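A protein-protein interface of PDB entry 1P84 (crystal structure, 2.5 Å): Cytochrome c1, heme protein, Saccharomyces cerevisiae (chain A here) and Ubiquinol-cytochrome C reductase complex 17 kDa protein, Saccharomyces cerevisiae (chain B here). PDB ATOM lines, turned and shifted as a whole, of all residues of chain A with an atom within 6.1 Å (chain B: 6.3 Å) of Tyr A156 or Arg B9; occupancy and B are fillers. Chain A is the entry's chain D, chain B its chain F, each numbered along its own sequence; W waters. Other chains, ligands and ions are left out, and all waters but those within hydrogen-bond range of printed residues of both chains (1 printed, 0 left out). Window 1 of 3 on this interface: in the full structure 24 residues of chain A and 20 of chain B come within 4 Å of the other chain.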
ATOM      1  N   HIS A   6     -10.149  19.182   7.993  1.00  0.00           N
ATOM      2  CA  HIS A   6     -11.188  18.990   6.977  1.00  0.00           C
ATOM      3  C   HIS A   6     -12.368  19.901   7.254  1.00  0.00           C
ATOM      4  O   HIS A   6     -12.923  20.498   6.338  1.00  0.00           O
ATOM      5  CB  HIS A   6     -11.700  17.542   6.955  1.00  0.00           C
ATOM      6  CG  HIS A   6     -10.791  16.573   6.258  1.00  0.00           C
ATOM      7  ND1 HIS A   6     -10.081  16.897   5.120  1.00  0.00           N
ATOM      8  CD2 HIS A   6     -10.500  15.276   6.525  1.00  0.00           C
ATOM      9  CE1 HIS A   6      -9.395  15.842   4.715  1.00  0.00           C
ATOM     10  NE2 HIS A   6      -9.630  14.845   5.550  1.00  0.00           N
ATOM     11  N   GLY A   7     -12.733  20.009   8.527  1.00  0.00           N
ATOM     12  CA  GLY A   7     -13.865  20.827   8.924  1.00  0.00           C
ATOM     13  C   GLY A   7     -15.051  19.927   9.210  1.00  0.00           C
ATOM     14  O   GLY A   7     -15.149  18.839   8.642  1.00  0.00           O
ATOM     15  N   LEU A   8     -15.943  20.361  10.095  1.00  0.00           N
ATOM     16  CA  LEU A   8     -17.118  19.564  10.448  1.00  0.00           C
ATOM     17  C   LEU A   8     -18.059  19.439   9.247  1.00  0.00           C
ATOM     18  O   LEU A   8     -18.387  20.430   8.595  1.00  0.00           O
ATOM     19  CB  LEU A   8     -17.853  20.207  11.628  1.00  0.00           C
ATOM     20  CG  LEU A   8     -18.579  19.352  12.674  1.00  0.00           C
ATOM     21  CD1 LEU A   8     -19.946  19.938  12.910  1.00  0.00           C
ATOM     22  CD2 LEU A   8     -18.700  17.906  12.246  1.00  0.00           C
ATOM     23  N   HIS A   9     -18.475  18.214   8.952  1.00  0.00           N
ATOM     24  CA  HIS A   9     -19.368  17.947   7.834  1.00  0.00           C
ATOM     25  C   HIS A   9     -20.734  18.580   8.052  1.00  0.00           C
ATOM     26  O   HIS A   9     -21.388  18.328   9.062  1.00  0.00           O
ATOM     27  CB  HIS A   9     -19.523  16.432   7.632  1.00  0.00           C
ATOM     28  CG  HIS A   9     -20.490  16.054   6.545  1.00  0.00           C
ATOM     29  ND1 HIS A   9     -21.738  15.524   6.806  1.00  0.00           N
ATOM     30  CD2 HIS A   9     -20.393  16.138   5.194  1.00  0.00           C
ATOM     31  CE1 HIS A   9     -22.369  15.299   5.665  1.00  0.00           C
ATOM     32  NE2 HIS A   9     -21.574  15.662   4.672  1.00  0.00           N
ATOM     33  N   ALA A  10     -21.167  19.388   7.091  1.00  0.00           N
ATOM     34  CA  ALA A  10     -22.464  20.042   7.171  1.00  0.00           C
ATOM     35  C   ALA A  10     -23.564  19.005   6.938  1.00  0.00           C
ATOM     36  O   ALA A  10     -23.463  18.184   6.035  1.00  0.00           O
ATOM     37  CB  ALA A  10     -22.553  21.160   6.145  1.00  0.00           C
ATOM     38  N   PRO A  11     -24.601  18.997   7.794  1.00  0.00           N
ATOM     39  CA  PRO A  11     -25.718  18.059   7.687  1.00  0.00           C
ATOM     40  C   PRO A  11     -26.685  18.503   6.608  1.00  0.00           C
ATOM     41  O   PRO A  11     -26.590  19.627   6.115  1.00  0.00           O
ATOM     42  CB  PRO A  11     -26.349  18.138   9.069  1.00  0.00           C
ATOM     43  CG  PRO A  11     -26.175  19.565   9.407  1.00  0.00           C
ATOM     44  CD  PRO A  11     -24.749  19.842   8.990  1.00  0.00           C
ATOM     45  N   TYR A  13     -30.105  19.847   5.552  1.00  0.00           N
ATOM     46  CA  TYR A  13     -31.366  20.531   5.863  1.00  0.00           C
ATOM     47  C   TYR A  13     -32.360  20.343   4.706  1.00  0.00           C
ATOM     48  O   TYR A  13     -31.958  20.201   3.548  1.00  0.00           O
ATOM     49  CB  TYR A  13     -31.120  22.012   6.127  1.00  0.00           C
ATOM     50  CG  TYR A  13     -30.357  22.250   7.405  1.00  0.00           C
ATOM     51  CD1 TYR A  13     -30.930  21.952   8.641  1.00  0.00           C
ATOM     52  CD2 TYR A  13     -29.053  22.734   7.383  1.00  0.00           C
ATOM     53  CE1 TYR A  13     -30.220  22.128   9.826  1.00  0.00           C
ATOM     54  CE2 TYR A  13     -28.331  22.917   8.562  1.00  0.00           C
ATOM     55  CZ  TYR A  13     -28.919  22.609   9.781  1.00  0.00           C
ATOM     56  OH  TYR A  13     -28.203  22.764  10.955  1.00  0.00           O
ATOM     57  N   TYR A 129     -23.749  24.036   3.607  1.00  0.00           N
ATOM     58  CA  TYR A 129     -22.525  24.599   4.158  1.00  0.00           C
ATOM     59  C   TYR A 129     -22.690  26.055   4.589  1.00  0.00           C
ATOM     60  O   TYR A 129     -22.353  26.398   5.715  1.00  0.00           O
ATOM     61  CB  TYR A 129     -21.364  24.476   3.158  1.00  0.00           C
ATOM     62  CG  TYR A 129     -20.134  25.234   3.579  1.00  0.00           C
ATOM     63  CD1 TYR A 129     -19.388  24.831   4.687  1.00  0.00           C
ATOM     64  CD2 TYR A 129     -19.757  26.395   2.922  1.00  0.00           C
ATOM     65  CE1 TYR A 129     -18.296  25.582   5.135  1.00  0.00           C
ATOM     66  CE2 TYR A 129     -18.670  27.152   3.365  1.00  0.00           C
ATOM     67  CZ  TYR A 129     -17.953  26.738   4.467  1.00  0.00           C
ATOM     68  OH  TYR A 129     -16.901  27.489   4.908  1.00  0.00           O
ATOM     69  N   SER A 132     -24.982  26.369   7.666  1.00  0.00           N
ATOM     70  CA  SER A 132     -24.290  25.816   8.811  1.00  0.00           C
ATOM     71  C   SER A 132     -23.177  26.700   9.327  1.00  0.00           C
ATOM     72  O   SER A 132     -23.000  26.832  10.531  1.00  0.00           O
ATOM     73  CB  SER A 132     -23.763  24.426   8.486  1.00  0.00           C
ATOM     74  OG  SER A 132     -24.843  23.518   8.317  1.00  0.00           O
ATOM     75  N   LEU A 133     -22.446  27.329   8.420  1.00  0.00           N
ATOM     76  CA  LEU A 133     -21.355  28.213   8.817  1.00  0.00           C
ATOM     77  C   LEU A 133     -21.910  29.435   9.565  1.00  0.00           C
ATOM     78  O   LEU A 133     -21.403  29.810  10.631  1.00  0.00           O
ATOM     79  CB  LEU A 133     -20.568  28.681   7.586  1.00  0.00           C
ATOM     80  CG  LEU A 133     -19.372  29.599   7.861  1.00  0.00           C
ATOM     81  CD1 LEU A 133     -18.128  28.774   8.141  1.00  0.00           C
ATOM     82  CD2 LEU A 133     -19.133  30.504   6.676  1.00  0.00           C
ATOM     83  N   THR A 135     -24.830  29.860  11.173  1.00  0.00           N
ATOM     84  CA  THR A 135     -25.479  29.559  12.447  1.00  0.00           C
ATOM     85  C   THR A 135     -24.671  28.631  13.353  1.00  0.00           C
ATOM     86  O   THR A 135     -25.192  28.117  14.349  1.00  0.00           O
ATOM     87  CB  THR A 135     -26.846  28.897  12.219  1.00  0.00           C
ATOM     88  OG1 THR A 135     -26.665  27.656  11.531  1.00  0.00           O
ATOM     89  CG2 THR A 135     -27.750  29.801  11.404  1.00  0.00           C
ATOM     90  N   GLY A 136     -23.398  28.440  13.030  1.00  0.00           N
ATOM     91  CA  GLY A 136     -22.576  27.537  13.811  1.00  0.00           C
ATOM     92  C   GLY A 136     -21.451  28.123  14.626  1.00  0.00           C
ATOM     93  O   GLY A 136     -20.488  27.421  14.907  1.00  0.00           O
ATOM     94  N   TYR A 137     -21.540  29.402  14.975  1.00  0.00           N
ATOM     95  CA  TYR A 137     -20.515  30.044  15.804  1.00  0.00           C
ATOM     96  C   TYR A 137     -20.819  29.751  17.279  1.00  0.00           C
ATOM     97  O   TYR A 137     -21.908  30.058  17.765  1.00  0.00           O
ATOM     98  CB  TYR A 137     -20.517  31.563  15.600  1.00  0.00           C
ATOM     99  CG  TYR A 137     -19.826  32.060  14.353  1.00  0.00           C
ATOM    100  CD1 TYR A 137     -20.525  32.210  13.159  1.00  0.00           C
ATOM    101  CD2 TYR A 137     -18.483  32.428  14.380  1.00  0.00           C
ATOM    102  CE1 TYR A 137     -19.907  32.718  12.023  1.00  0.00           C
ATOM    103  CE2 TYR A 137     -17.854  32.936  13.254  1.00  0.00           C
ATOM    104  CZ  TYR A 137     -18.572  33.078  12.079  1.00  0.00           C
ATOM    105  OH  TYR A 137     -17.956  33.582  10.963  1.00  0.00           O
ATOM    106  N   ASN A 154     -15.179  28.467  14.305  1.00  0.00           N
ATOM    107  CA  ASN A 154     -16.365  27.929  13.653  1.00  0.00           C
ATOM    108  C   ASN A 154     -15.909  26.526  13.269  1.00  0.00           C
ATOM    109  O   ASN A 154     -14.864  26.351  12.634  1.00  0.00           O
ATOM    110  CB  ASN A 154     -16.693  28.750  12.407  1.00  0.00           C
ATOM    111  CG  ASN A 154     -18.061  28.445  11.858  1.00  0.00           C
ATOM    112  OD1 ASN A 154     -18.421  27.282  11.653  1.00  0.00           O
ATOM    113  ND2 ASN A 154     -18.841  29.490  11.614  1.00  0.00           N
ATOM    114  N   PRO A 155     -16.659  25.502  13.688  1.00  0.00           N
ATOM    115  CA  PRO A 155     -16.272  24.127  13.365  1.00  0.00           C
ATOM    116  C   PRO A 155     -16.444  23.715  11.897  1.00  0.00           C
ATOM    117  O   PRO A 155     -15.705  22.861  11.401  1.00  0.00           O
ATOM    118  CB  PRO A 155     -17.165  23.310  14.294  1.00  0.00           C
ATOM    119  CG  PRO A 155     -18.425  24.130  14.339  1.00  0.00           C
ATOM    120  CD  PRO A 155     -17.891  25.532  14.493  1.00  0.00           C
ATOM    121  N   TYR A 156     -17.398  24.331  11.203  1.00  0.00           N
ATOM    122  CA  TYR A 156     -17.667  23.988   9.807  1.00  0.00           C
ATOM    123  C   TYR A 156     -16.621  24.493   8.822  1.00  0.00           C
ATOM    124  O   TYR A 156     -16.468  23.936   7.738  1.00  0.00           O
ATOM    125  CB  TYR A 156     -19.066  24.452   9.413  1.00  0.00           C
ATOM    126  CG  TYR A 156     -20.139  23.844  10.287  1.00  0.00           C
ATOM    127  CD1 TYR A 156     -20.661  24.544  11.377  1.00  0.00           C
ATOM    128  CD2 TYR A 156     -20.617  22.562  10.041  1.00  0.00           C
ATOM    129  CE1 TYR A 156     -21.632  23.980  12.198  1.00  0.00           C
ATOM    130  CE2 TYR A 156     -21.591  21.987  10.861  1.00  0.00           C
ATOM    131  CZ  TYR A 156     -22.090  22.706  11.939  1.00  0.00           C
ATOM    132  OH  TYR A 156     -23.032  22.136  12.760  1.00  0.00           O
ATOM    133  N   PHE A 157     -15.889  25.531   9.209  1.00  0.00           N
ATOM    134  CA  PHE A 157     -14.842  26.091   8.365  1.00  0.00           C
ATOM    135  C   PHE A 157     -13.566  25.256   8.558  1.00  0.00           C
ATOM    136  O   PHE A 157     -13.231  24.880   9.679  1.00  0.00           O
ATOM    137  CB  PHE A 157     -14.601  27.550   8.755  1.00  0.00           C
ATOM    138  CG  PHE A 157     -13.648  28.281   7.851  1.00  0.00           C
ATOM    139  CD1 PHE A 157     -14.067  28.755   6.606  1.00  0.00           C
ATOM    140  CD2 PHE A 157     -12.338  28.521   8.252  1.00  0.00           C
ATOM    141  CE1 PHE A 157     -13.192  29.459   5.779  1.00  0.00           C
ATOM    142  CE2 PHE A 157     -11.454  29.223   7.432  1.00  0.00           C
ATOM    143  CZ  PHE A 157     -11.879  29.695   6.197  1.00  0.00           C
ATOM    144  N   PRO A 158     -12.865  24.913   7.456  1.00  0.00           N
ATOM    145  CA  PRO A 158     -11.627  24.121   7.502  1.00  0.00           C
ATOM    146  C   PRO A 158     -10.564  24.794   8.356  1.00  0.00           C
ATOM    147  O   PRO A 158     -10.250  25.967   8.156  1.00  0.00           O
ATOM    148  CB  PRO A 158     -11.196  24.089   6.034  1.00  0.00           C
ATOM    149  CG  PRO A 158     -12.493  24.146   5.302  1.00  0.00           C
ATOM    150  CD  PRO A 158     -13.227  25.219   6.060  1.00  0.00           C
ATOM    151  N   GLN B   4     -35.131  29.147  16.672  1.00  0.00           N
ATOM    152  CA  GLN B   4     -35.548  27.761  16.458  1.00  0.00           C
ATOM    153  C   GLN B   4     -34.444  26.705  16.482  1.00  0.00           C
ATOM    154  O   GLN B   4     -34.683  25.571  16.904  1.00  0.00           O
ATOM    155  CB  GLN B   4     -36.346  27.638  15.156  1.00  0.00           C
ATOM    156  CG  GLN B   4     -37.593  28.509  15.080  1.00  0.00           C
ATOM    157  CD  GLN B   4     -37.340  29.877  14.467  1.00  0.00           C
ATOM    158  OE1 GLN B   4     -38.226  30.450  13.831  1.00  0.00           O
ATOM    159  NE2 GLN B   4     -36.127  30.399  14.636  1.00  0.00           N
ATOM    160  N   LEU B   5     -33.249  27.059  16.012  1.00  0.00           N
ATOM    161  CA  LEU B   5     -32.139  26.115  16.009  1.00  0.00           C
ATOM    162  C   LEU B   5     -31.602  25.924  17.428  1.00  0.00           C
ATOM    163  O   LEU B   5     -31.403  24.794  17.875  1.00  0.00           O
ATOM    164  CB  LEU B   5     -31.020  26.585  15.073  1.00  0.00           C
ATOM    165  CG  LEU B   5     -29.785  25.680  14.974  1.00  0.00           C
ATOM    166  CD1 LEU B   5     -30.151  24.328  14.409  1.00  0.00           C
ATOM    167  CD2 LEU B   5     -28.739  26.343  14.118  1.00  0.00           C
ATOM    168  N   GLU B   6     -31.377  27.031  18.136  1.00  0.00           N
ATOM    169  CA  GLU B   6     -30.879  26.972  19.513  1.00  0.00           C
ATOM    170  C   GLU B   6     -31.850  26.222  20.411  1.00  0.00           C
ATOM    171  O   GLU B   6     -31.448  25.559  21.366  1.00  0.00           O
ATOM    172  CB  GLU B   6     -30.657  28.374  20.074  1.00  0.00           C
ATOM    173  CG  GLU B   6     -29.419  29.053  19.540  1.00  0.00           C
ATOM    174  CD  GLU B   6     -28.640  29.751  20.633  1.00  0.00           C
ATOM    175  OE1 GLU B   6     -28.898  30.954  20.870  1.00  0.00           O
ATOM    176  OE2 GLU B   6     -27.784  29.088  21.260  1.00  0.00           O
ATOM    177  N   ASP B   7     -33.132  26.351  20.094  1.00  0.00           N
ATOM    178  CA  ASP B   7     -34.194  25.689  20.830  1.00  0.00           C
ATOM    179  C   ASP B   7     -34.020  24.180  20.672  1.00  0.00           C
ATOM    180  O   ASP B   7     -33.957  23.458  21.662  1.00  0.00           O
ATOM    181  CB  ASP B   7     -35.548  26.136  20.275  1.00  0.00           C
ATOM    182  CG  ASP B   7     -36.718  25.610  21.079  1.00  0.00           C
ATOM    183  OD1 ASP B   7     -37.166  26.327  22.002  1.00  0.00           O
ATOM    184  OD2 ASP B   7     -37.204  24.495  20.771  1.00  0.00           O
ATOM    185  N   LEU B   8     -33.903  23.719  19.426  1.00  0.00           N
ATOM    186  CA  LEU B   8     -33.728  22.298  19.131  1.00  0.00           C
ATOM    187  C   LEU B   8     -32.401  21.718  19.624  1.00  0.00           C
ATOM    188  O   LEU B   8     -32.334  20.543  19.991  1.00  0.00           O
ATOM    189  CB  LEU B   8     -33.903  22.031  17.635  1.00  0.00           C
ATOM    190  CG  LEU B   8     -35.354  21.930  17.168  1.00  0.00           C
ATOM    191  CD1 LEU B   8     -35.415  21.845  15.661  1.00  0.00           C
ATOM    192  CD2 LEU B   8     -36.007  20.714  17.797  1.00  0.00           C
ATOM    193  N   ARG B   9     -31.345  22.528  19.616  1.00  0.00           N
ATOM    194  CA  ARG B   9     -30.043  22.074  20.095  1.00  0.00           C
ATOM    195  C   ARG B   9     -30.134  21.817  21.589  1.00  0.00           C
ATOM    196  O   ARG B   9     -29.771  20.739  22.068  1.00  0.00           O
ATOM    197  CB  ARG B   9     -28.956  23.104  19.797  1.00  0.00           C
ATOM    198  CG  ARG B   9     -28.449  23.004  18.382  1.00  0.00           C
ATOM    199  CD  ARG B   9     -27.327  23.980  18.049  1.00  0.00           C
ATOM    200  NE  ARG B   9     -26.820  23.687  16.708  1.00  0.00           N
ATOM    201  CZ  ARG B   9     -26.183  24.547  15.918  1.00  0.00           C
ATOM    202  NH1 ARG B   9     -25.777  24.144  14.722  1.00  0.00           N
ATOM    203  NH2 ARG B   9     -25.949  25.796  16.310  1.00  0.00           N
ATOM    204  N   GLU B  10     -30.690  22.795  22.306  1.00  0.00           N
ATOM    205  CA  GLU B  10     -30.874  22.718  23.751  1.00  0.00           C
ATOM    206  C   GLU B  10     -31.686  21.473  24.107  1.00  0.00           C
ATOM    207  O   GLU B  10     -31.296  20.698  24.982  1.00  0.00           O
ATOM    208  CB  GLU B  10     -31.586  23.978  24.255  1.00  0.00           C
ATOM    209  CG  GLU B  10     -31.331  24.296  25.722  1.00  0.00           C
ATOM    210  CD  GLU B  10     -29.850  24.443  26.034  1.00  0.00           C
ATOM    211  OE1 GLU B  10     -29.136  25.132  25.264  1.00  0.00           O
ATOM    212  OE2 GLU B  10     -29.396  23.853  27.041  1.00  0.00           O
ATOM    213  N   HIS B  11     -32.792  21.265  23.398  1.00  0.00           N
ATOM    214  CA  HIS B  11     -33.638  20.107  23.636  1.00  0.00           C
ATOM    215  C   HIS B  11     -32.853  18.808  23.500  1.00  0.00           C
ATOM    216  O   HIS B  11     -33.051  17.884  24.290  1.00  0.00           O
ATOM    217  CB  HIS B  11     -34.827  20.094  22.672  1.00  0.00           C
ATOM    218  CG  HIS B  11     -35.549  18.782  22.618  1.00  0.00           C
ATOM    219  ND1 HIS B  11     -36.637  18.495  23.415  1.00  0.00           N
ATOM    220  CD2 HIS B  11     -35.326  17.669  21.877  1.00  0.00           C
ATOM    221  CE1 HIS B  11     -37.050  17.265  23.170  1.00  0.00           C
ATOM    222  NE2 HIS B  11     -36.271  16.740  22.239  1.00  0.00           N
ATOM    223  N   PHE B  12     -31.955  18.742  22.516  1.00  0.00           N
ATOM    224  CA  PHE B  12     -31.170  17.528  22.289  1.00  0.00           C
ATOM    225  C   PHE B  12     -29.939  17.332  23.158  1.00  0.00           C
ATOM    226  O   PHE B  12     -29.527  16.195  23.397  1.00  0.00           O
ATOM    227  CB  PHE B  12     -30.855  17.342  20.804  1.00  0.00           C
ATOM    228  CG  PHE B  12     -31.997  16.754  20.030  1.00  0.00           C
ATOM    229  CD1 PHE B  12     -32.813  17.555  19.238  1.00  0.00           C
ATOM    230  CD2 PHE B  12     -32.299  15.401  20.151  1.00  0.00           C
ATOM    231  CE1 PHE B  12     -33.921  17.014  18.586  1.00  0.00           C
ATOM    232  CE2 PHE B  12     -33.404  14.852  19.501  1.00  0.00           C
ATOM    233  CZ  PHE B  12     -34.217  15.658  18.719  1.00  0.00           C
ATOM    234  N   LYS B  13     -29.372  18.424  23.658  1.00  0.00           N
ATOM    235  CA  LYS B  13     -28.214  18.326  24.538  1.00  0.00           C
ATOM    236  C   LYS B  13     -28.655  17.653  25.849  1.00  0.00           C
ATOM    237  O   LYS B  13     -27.824  17.167  26.619  1.00  0.00           O
ATOM    238  CB  LYS B  13     -27.650  19.718  24.831  1.00  0.00           C
ATOM    239  CG  LYS B  13     -27.283  20.512  23.581  1.00  0.00           C
ATOM    240  CD  LYS B  13     -27.027  22.002  23.863  1.00  0.00           C
ATOM    241  CE  LYS B  13     -25.574  22.296  24.220  1.00  0.00           C
ATOM    242  NZ  LYS B  13     -25.106  21.550  25.422  1.00  0.00           N
ATOM    243  N   ASN B  14     -29.971  17.586  26.061  1.00  0.00           N
ATOM    244  CA  ASN B  14     -30.557  16.995  27.265  1.00  0.00           C
ATOM    245  C   ASN B  14     -31.181  15.605  27.116  1.00  0.00           C
ATOM    246  O   ASN B  14     -32.083  15.246  27.873  1.00  0.00           O
ATOM    247  CB  ASN B  14     -31.576  17.958  27.901  1.00  0.00           C
ATOM    248  CG  ASN B  14     -30.917  19.170  28.546  1.00  0.00           C
ATOM    249  OD1 ASN B  14     -30.117  19.039  29.479  1.00  0.00           O
ATOM    250  ND2 ASN B  14     -31.250  20.358  28.048  1.00  0.00           N
ATOM    251  N   PHE B  55     -16.509  17.791  18.230  1.00  0.00           N
ATOM    252  CA  PHE B  55     -17.076  17.373  16.948  1.00  0.00           C
ATOM    253  C   PHE B  55     -18.117  16.260  17.111  1.00  0.00           C
ATOM    254  O   PHE B  55     -19.129  16.251  16.403  1.00  0.00           O
ATOM    255  CB  PHE B  55     -15.975  16.923  15.977  1.00  0.00           C
ATOM    256  CG  PHE B  55     -15.402  18.033  15.131  1.00  0.00           C
ATOM    257  CD1 PHE B  55     -14.923  17.763  13.854  1.00  0.00           C
ATOM    258  CD2 PHE B  55     -15.318  19.337  15.608  1.00  0.00           C
ATOM    259  CE1 PHE B  55     -14.363  18.777  13.059  1.00  0.00           C
ATOM    260  CE2 PHE B  55     -14.757  20.360  14.822  1.00  0.00           C
ATOM    261  CZ  PHE B  55     -14.280  20.074  13.549  1.00  0.00           C
ATOM    262  N   GLN B  58     -21.291  17.998  18.443  1.00  0.00           N
ATOM    263  CA  GLN B  58     -21.868  18.758  17.339  1.00  0.00           C
ATOM    264  C   GLN B  58     -22.496  17.863  16.276  1.00  0.00           C
ATOM    265  O   GLN B  58     -23.589  18.146  15.778  1.00  0.00           O
ATOM    266  CB  GLN B  58     -20.818  19.650  16.700  1.00  0.00           C
ATOM    267  CG  GLN B  58     -21.428  20.815  15.952  1.00  0.00           C
ATOM    268  CD  GLN B  58     -22.193  21.762  16.868  1.00  0.00           C
ATOM    269  OE1 GLN B  58     -21.915  21.847  18.076  1.00  0.00           O
ATOM    270  NE2 GLN B  58     -23.160  22.481  16.300  1.00  0.00           N
ATOM    271  N   LEU B  61     -25.796  16.479  17.433  1.00  0.00           N
ATOM    272  CA  LEU B  61     -26.770  17.558  17.385  1.00  0.00           C
ATOM    273  C   LEU B  61     -27.243  17.800  15.960  1.00  0.00           C
ATOM    274  O   LEU B  61     -28.449  17.902  15.706  1.00  0.00           O
ATOM    275  CB  LEU B  61     -26.173  18.843  17.963  1.00  0.00           C
ATOM    276  CG  LEU B  61     -25.743  18.777  19.432  1.00  0.00           C
ATOM    277  CD1 LEU B  61     -25.150  20.116  19.855  1.00  0.00           C
ATOM    278  CD2 LEU B  61     -26.938  18.398  20.308  1.00  0.00           C
ATOM    279  N   ASP B  62     -26.285  17.886  15.034  1.00  0.00           N
ATOM    280  CA  ASP B  62     -26.594  18.100  13.626  1.00  0.00           C
ATOM    281  C   ASP B  62     -27.506  16.994  13.113  1.00  0.00           C
ATOM    282  O   ASP B  62     -28.516  17.265  12.468  1.00  0.00           O
ATOM    283  CB  ASP B  62     -25.311  18.134  12.790  1.00  0.00           C
ATOM    284  CG  ASP B  62     -24.580  19.461  12.880  1.00  0.00           C
ATOM    285  OD1 ASP B  62     -25.202  20.465  13.282  1.00  0.00           O
ATOM    286  OD2 ASP B  62     -23.378  19.505  12.528  1.00  0.00           O
ATOM    287  N   THR B  65     -31.055  17.676  14.647  1.00  0.00           N
ATOM    288  CA  THR B  65     -31.685  18.941  14.301  1.00  0.00           C
ATOM    289  C   THR B  65     -31.901  19.239  12.819  1.00  0.00           C
ATOM    290  O   THR B  65     -32.831  19.965  12.464  1.00  0.00           O
ATOM    291  CB  THR B  65     -30.938  20.123  14.945  1.00  0.00           C
ATOM    292  OG1 THR B  65     -29.653  20.281  14.333  1.00  0.00           O
ATOM    293  CG2 THR B  65     -30.749  19.878  16.426  1.00  0.00           C
HETATM  294  O   HOH W   1     -22.669  16.971  10.987  1.00  0.00           O
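Water W1 bridges the backbone carbonyl oxygen (O) of His A9 (2.7 Å) and the side-chain carboxylate (OD2) of Asp B62 (3.0 Å).
Hydrophobic or aromatic side chains of chain A within 4 Å of the printed part of chain B: Leu A8, Pro A11, Pro A155 and Tyr A156.
Along chain A the printed residues that touch a printed residue of chain B span positions 8 to 156.
Of the 16 printed residues of chain B, 5 touch a printed residue of chain A.
Hydrophobic or aromatic side chains of chain B that line the printed part of chain A: Leu B5 and Phe B55.
Among the printed residues, 10 pairs touch across the chains.
OH of Tyr A156 lies within hydrogen-bond range of OD2 of Asp B62, at 2.7 Å.
NH2 of Arg B9 lies within hydrogen-bond range of O of Thr A135, at 3.1 Å.
The side-chain amide nitrogen (NE2) of Gln B58 lies close to the guanidinium group (NH1) of Arg B9 (3.5 Å).
N of Tyr A156 is in hydrogen-bond range of OD1 of Asn A154.
The backbone NH (N) of Leu A8 is in hydrogen-bond range of the backbone carbonyl oxygen (O) of Pro A155, 2.8 Å away.
The guanidinium group (NH1) of Arg B9 lies within salt-bridge range of the side-chain carboxylate (OD1) of Asp B62.
Leu A8 touches Phe B55.
CD1 of Leu A8 touches CG of Gln B58, at 3.5 Å.
OD2 of Asp B62 touches CD1 of Leu A8 (3.5 Å).
Asp B62 touches Pro A11 (CB to CG, 3.8 Å).
Leu B5 touches Thr A135.
Pro A155 touches Phe B55 (O to CZ, 3.8 Å).
Arg B9 touches Tyr A156.
NE2 of Gln B58 touches OH of Tyr A156 (3.6 Å).
Tyr A156 touches just these residues of chain B: Arg B9 (3.9 Å), Gln B58 (3.6 Å) and Asp B62 (2.7 Å).
Arg B9 touches just these residues of chain A: Thr A135 and Tyr A156.
Printed residues of chain B within 4 Å of Thr A135: Leu B5 (3.6 Å) and Arg B9 (3.1 Å).
Of the printed residues of chain A, Phe B55 touches Leu A8 (3.7 Å) and Pro A155 (3.8 Å).
Printed residues of chain B within 4 Å of Leu A8: Phe B55 (3.7 Å), Gln B58 (3.5 Å) and Asp B62 (3.5 Å).
Gly A136 touches none of the printed residues of chain B.
Tyr A13 touches none of the printed residues of chain B.
The nearest residue of chain A that does not touch Arg B9 is Gly A136 (4.5 Å).
The nearest printed residue of chain B that does not touch Pro A11 is Thr B65 (6.1 Å).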
